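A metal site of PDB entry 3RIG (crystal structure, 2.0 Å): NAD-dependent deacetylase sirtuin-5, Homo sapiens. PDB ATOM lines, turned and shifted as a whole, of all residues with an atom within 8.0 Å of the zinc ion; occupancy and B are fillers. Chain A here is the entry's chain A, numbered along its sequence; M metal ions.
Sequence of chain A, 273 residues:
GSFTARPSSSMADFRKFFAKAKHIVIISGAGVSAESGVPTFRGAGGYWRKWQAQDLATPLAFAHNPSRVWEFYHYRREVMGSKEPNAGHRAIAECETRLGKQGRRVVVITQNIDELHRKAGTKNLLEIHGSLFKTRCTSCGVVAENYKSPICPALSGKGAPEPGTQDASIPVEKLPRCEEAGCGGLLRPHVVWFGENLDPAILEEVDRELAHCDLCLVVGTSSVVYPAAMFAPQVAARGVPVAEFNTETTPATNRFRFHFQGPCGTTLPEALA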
ATOM      1  N   ARG A 136      25.371  18.968 -15.151  1.00  0.00           N
ATOM      2  CA  ARG A 136      24.081  18.971 -14.555  1.00  0.00           C
ATOM      3  C   ARG A 136      23.953  20.266 -13.761  1.00  0.00           C
ATOM      4  O   ARG A 136      24.864  20.669 -13.069  1.00  0.00           O
ATOM      5  CB  ARG A 136      23.921  17.779 -13.628  1.00  0.00           C
ATOM      6  CG  ARG A 136      22.554  17.809 -12.928  1.00  0.00           C
ATOM      7  CD  ARG A 136      22.201  16.501 -12.197  1.00  0.00           C
ATOM      8  NE  ARG A 136      22.874  16.289 -10.905  1.00  0.00           N
ATOM      9  CZ  ARG A 136      23.937  15.503 -10.745  1.00  0.00           C
ATOM     10  NH1 ARG A 136      24.477  14.917 -11.801  1.00  0.00           N
ATOM     11  NH2 ARG A 136      24.452  15.272  -9.534  1.00  0.00           N
ATOM     12  N   CYS A 137      22.814  20.895 -13.854  1.00  0.00           N
ATOM     13  CA  CYS A 137      22.622  22.156 -13.155  1.00  0.00           C
ATOM     14  C   CYS A 137      22.261  21.943 -11.679  1.00  0.00           C
ATOM     15  O   CYS A 137      21.322  21.197 -11.395  1.00  0.00           O
ATOM     16  CB  CYS A 137      21.543  22.972 -13.855  1.00  0.00           C
ATOM     17  SG  CYS A 137      21.012  24.476 -12.992  1.00  0.00           S
ATOM     18  N   THR A 138      22.943  22.632 -10.754  1.00  0.00           N
ATOM     19  CA  THR A 138      22.704  22.421  -9.320  1.00  0.00           C
ATOM     20  C   THR A 138      21.443  23.125  -8.857  1.00  0.00           C
ATOM     21  O   THR A 138      21.051  22.985  -7.693  1.00  0.00           O
ATOM     22  CB  THR A 138      23.876  22.891  -8.461  1.00  0.00           C
ATOM     23  OG1 THR A 138      24.156  24.241  -8.813  1.00  0.00           O
ATOM     24  CG2 THR A 138      25.125  22.009  -8.740  1.00  0.00           C
ATOM     25  N   SER A 139      20.820  23.883  -9.752  1.00  0.00           N
ATOM     26  CA  SER A 139      19.592  24.622  -9.442  1.00  0.00           C
ATOM     27  C   SER A 139      18.346  23.881  -9.923  1.00  0.00           C
ATOM     28  O   SER A 139      17.487  23.532  -9.120  1.00  0.00           O
ATOM     29  CB  SER A 139      19.621  26.013 -10.072  1.00  0.00           C
ATOM     30  OG  SER A 139      20.410  26.891  -9.293  1.00  0.00           O
ATOM     31  N   CYS A 140      18.238  23.673 -11.233  1.00  0.00           N
ATOM     32  CA  CYS A 140      17.044  23.036 -11.762  1.00  0.00           C
ATOM     33  C   CYS A 140      17.241  21.571 -12.138  1.00  0.00           C
ATOM     34  O   CYS A 140      16.295  20.907 -12.591  1.00  0.00           O
ATOM     35  CB  CYS A 140      16.547  23.785 -12.981  1.00  0.00           C
ATOM     36  SG  CYS A 140      17.546  23.400 -14.427  1.00  0.00           S
ATOM     37  N   GLY A 141      18.452  21.066 -12.016  1.00  0.00           N
ATOM     38  CA  GLY A 141      18.697  19.666 -12.293  1.00  0.00           C
ATOM     39  C   GLY A 141      18.810  19.175 -13.732  1.00  0.00           C
ATOM     40  O   GLY A 141      19.083  17.974 -13.914  1.00  0.00           O
ATOM     41  N   VAL A 142      18.636  20.044 -14.733  1.00  0.00           N
ATOM     42  CA  VAL A 142      18.783  19.606 -16.150  1.00  0.00           C
ATOM     43  C   VAL A 142      20.190  19.069 -16.463  1.00  0.00           C
ATOM     44  O   VAL A 142      21.201  19.634 -15.996  1.00  0.00           O
ATOM     45  CB  VAL A 142      18.320  20.690 -17.238  1.00  0.00           C
ATOM     46  CG1 VAL A 142      19.388  21.661 -17.549  1.00  0.00           C
ATOM     47  CG2 VAL A 142      18.053  20.010 -18.551  1.00  0.00           C
ATOM     48  N   VAL A 143      20.234  17.998 -17.245  1.00  0.00           N
ATOM     49  CA  VAL A 143      21.466  17.403 -17.657  1.00  0.00           C
ATOM     50  C   VAL A 143      21.530  17.698 -19.125  1.00  0.00           C
ATOM     51  O   VAL A 143      20.477  17.638 -19.798  1.00  0.00           O
ATOM     52  CB  VAL A 143      21.470  15.841 -17.426  1.00  0.00           C
ATOM     53  CG1 VAL A 143      22.717  15.175 -18.116  1.00  0.00           C
ATOM     54  CG2 VAL A 143      21.395  15.543 -15.926  1.00  0.00           C
ATOM     55  N   ARG A 177      27.621  28.124 -16.200  1.00  0.00           N
ATOM     56  CA  ARG A 177      26.265  28.473 -15.726  1.00  0.00           C
ATOM     57  C   ARG A 177      25.156  27.880 -16.599  1.00  0.00           C
ATOM     58  O   ARG A 177      25.403  27.600 -17.755  1.00  0.00           O
ATOM     59  CB  ARG A 177      26.087  30.012 -15.622  1.00  0.00           C
ATOM     60  CG  ARG A 177      27.133  30.763 -14.712  1.00  0.00           C
ATOM     61  CD  ARG A 177      27.251  30.211 -13.321  1.00  0.00           C
ATOM     62  NE  ARG A 177      26.065  30.510 -12.515  1.00  0.00           N
ATOM     63  CZ  ARG A 177      26.093  30.658 -11.203  1.00  0.00           C
ATOM     64  NH1 ARG A 177      27.229  30.507 -10.535  1.00  0.00           N
ATOM     65  NH2 ARG A 177      24.992  30.953 -10.554  1.00  0.00           N
ATOM     66  N   CYS A 178      23.955  27.678 -16.031  1.00  0.00           N
ATOM     67  CA  CYS A 178      22.800  26.994 -16.713  1.00  0.00           C
ATOM     68  C   CYS A 178      22.133  27.966 -17.692  1.00  0.00           C
ATOM     69  O   CYS A 178      21.808  29.077 -17.347  1.00  0.00           O
ATOM     70  CB  CYS A 178      21.792  26.466 -15.646  1.00  0.00           C
ATOM     71  SG  CYS A 178      20.189  25.527 -16.094  1.00  0.00           S
ATOM     72  N   GLU A 179      21.900  27.503 -18.924  1.00  0.00           N
ATOM     73  CA  GLU A 179      21.309  28.307 -19.963  1.00  0.00           C
ATOM     74  C   GLU A 179      19.766  28.181 -20.087  1.00  0.00           C
ATOM     75  O   GLU A 179      19.127  28.903 -20.855  1.00  0.00           O
ATOM     76  CB  GLU A 179      22.078  28.097 -21.278  1.00  0.00           C
ATOM     77  CG  GLU A 179      23.481  28.810 -21.265  1.00  0.00           C
ATOM     78  CD  GLU A 179      24.366  28.496 -22.475  1.00  0.00           C
ATOM     79  OE1 GLU A 179      24.793  27.331 -22.633  1.00  0.00           O
ATOM     80  OE2 GLU A 179      24.626  29.426 -23.282  1.00  0.00           O
ATOM     81  N   GLU A 180      19.153  27.302 -19.304  1.00  0.00           N
ATOM     82  CA  GLU A 180      17.680  27.213 -19.269  1.00  0.00           C
ATOM     83  C   GLU A 180      16.989  28.514 -18.756  1.00  0.00           C
ATOM     84  O   GLU A 180      17.478  29.197 -17.840  1.00  0.00           O
ATOM     85  CB  GLU A 180      17.226  25.975 -18.465  1.00  0.00           C
ATOM     86  CG  GLU A 180      17.828  24.632 -18.951  1.00  0.00           C
ATOM     87  CD  GLU A 180      17.190  24.098 -20.225  1.00  0.00           C
ATOM     88  OE1 GLU A 180      15.930  24.041 -20.266  1.00  0.00           O
ATOM     89  OE2 GLU A 180      17.935  23.747 -21.173  1.00  0.00           O
ATOM     90  N   ALA A 181      15.860  28.866 -19.389  1.00  0.00           N
ATOM     91  CA  ALA A 181      15.063  30.050 -19.107  1.00  0.00           C
ATOM     92  C   ALA A 181      14.768  30.344 -17.621  1.00  0.00           C
ATOM     93  O   ALA A 181      14.256  29.489 -16.875  1.00  0.00           O
ATOM     94  CB  ALA A 181      13.759  30.013 -19.905  1.00  0.00           C
ATOM     95  N   GLY A 182      15.087  31.557 -17.186  1.00  0.00           N
ATOM     96  CA  GLY A 182      14.848  31.970 -15.799  1.00  0.00           C
ATOM     97  C   GLY A 182      15.785  31.326 -14.785  1.00  0.00           C
ATOM     98  O   GLY A 182      15.591  31.463 -13.569  1.00  0.00           O
ATOM     99  N   CYS A 183      16.808  30.636 -15.289  1.00  0.00           N
ATOM    100  CA  CYS A 183      17.725  29.886 -14.415  1.00  0.00           C
ATOM    101  C   CYS A 183      19.136  30.485 -14.174  1.00  0.00           C
ATOM    102  O   CYS A 183      19.390  31.053 -13.127  1.00  0.00           O
ATOM    103  CB  CYS A 183      17.840  28.439 -14.904  1.00  0.00           C
ATOM    104  SG  CYS A 183      18.673  27.431 -13.687  1.00  0.00           S
ATOM    105  N   GLY A 184      20.069  30.300 -15.104  1.00  0.00           N
ATOM    106  CA  GLY A 184      21.491  30.612 -14.866  1.00  0.00           C
ATOM    107  C   GLY A 184      22.167  30.035 -13.613  1.00  0.00           C
ATOM    108  O   GLY A 184      23.052  30.664 -13.023  1.00  0.00           O
ATOM    109  N   GLY A 185      21.779  28.824 -13.193  1.00  0.00           N
ATOM    110  CA  GLY A 185      22.350  28.254 -11.952  1.00  0.00           C
ATOM    111  C   GLY A 185      23.767  27.762 -12.216  1.00  0.00           C
ATOM    112  O   GLY A 185      24.183  27.678 -13.366  1.00  0.00           O
ATOM    113  N   LEU A 186      24.495  27.405 -11.177  1.00  0.00           N
ATOM    114  CA  LEU A 186      25.839  26.862 -11.316  1.00  0.00           C
ATOM    115  C   LEU A 186      25.842  25.412 -11.830  1.00  0.00           C
ATOM    116  O   LEU A 186      25.148  24.580 -11.304  1.00  0.00           O
ATOM    117  CB  LEU A 186      26.592  26.952  -9.976  1.00  0.00           C
ATOM    118  CG  LEU A 186      27.933  26.204  -9.833  1.00  0.00           C
ATOM    119  CD1 LEU A 186      28.999  26.866 -10.738  1.00  0.00           C
ATOM    120  CD2 LEU A 186      28.389  26.130  -8.377  1.00  0.00           C
ATOM    121  N   LEU A 187      26.619  25.114 -12.865  1.00  0.00           N
ATOM    122  CA  LEU A 187      26.695  23.723 -13.336  1.00  0.00           C
ATOM    123  C   LEU A 187      27.750  22.972 -12.566  1.00  0.00           C
ATOM    124  O   LEU A 187      28.703  23.568 -12.071  1.00  0.00           O
ATOM    125  CB  LEU A 187      27.000  23.669 -14.838  1.00  0.00           C
ATOM    126  CG  LEU A 187      26.080  24.448 -15.761  1.00  0.00           C
ATOM    127  CD1 LEU A 187      26.486  24.237 -17.205  1.00  0.00           C
ATOM    128  CD2 LEU A 187      24.587  24.059 -15.585  1.00  0.00           C
HETATM  129 ZN    ZN M   1      19.460  25.249 -14.326  1.00  0.00          ZN
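The backbone NH (N) of Cys 178 is in hydrogen-bond range of the backbone carbonyl oxygen (O) of Gly 185.
O of Cys 178 lies close to N of Gly 184 (3.1 Å).
The backbone NH (N) of Ser 139 lies close to the side-chain sulfur (SG) of Cys 137.
The backbone NH (N) of Cys 137 sits at hydrogen-bond distance from the backbone carbonyl oxygen (O) of Val 142 (3.0 Å).
SG of Cys 183 lies close to N of Gly 185 (3.4 Å).
SG of Cys 140 sits close to N of Val 142 (3.5 Å).
Of the 19 residues printed, 4 come within 4 Å of the zinc ion.
The zinc ion is bound by the side-chain sulfur (SG) of Cys 178 (1.9 Å), the side-chain sulfur (SG) of Cys 137 (2.2 Å), the side-chain sulfur (SG) of Cys 183 (2.4 Å) and the side-chain sulfur (SG) of Cys 140 (2.7 Å).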
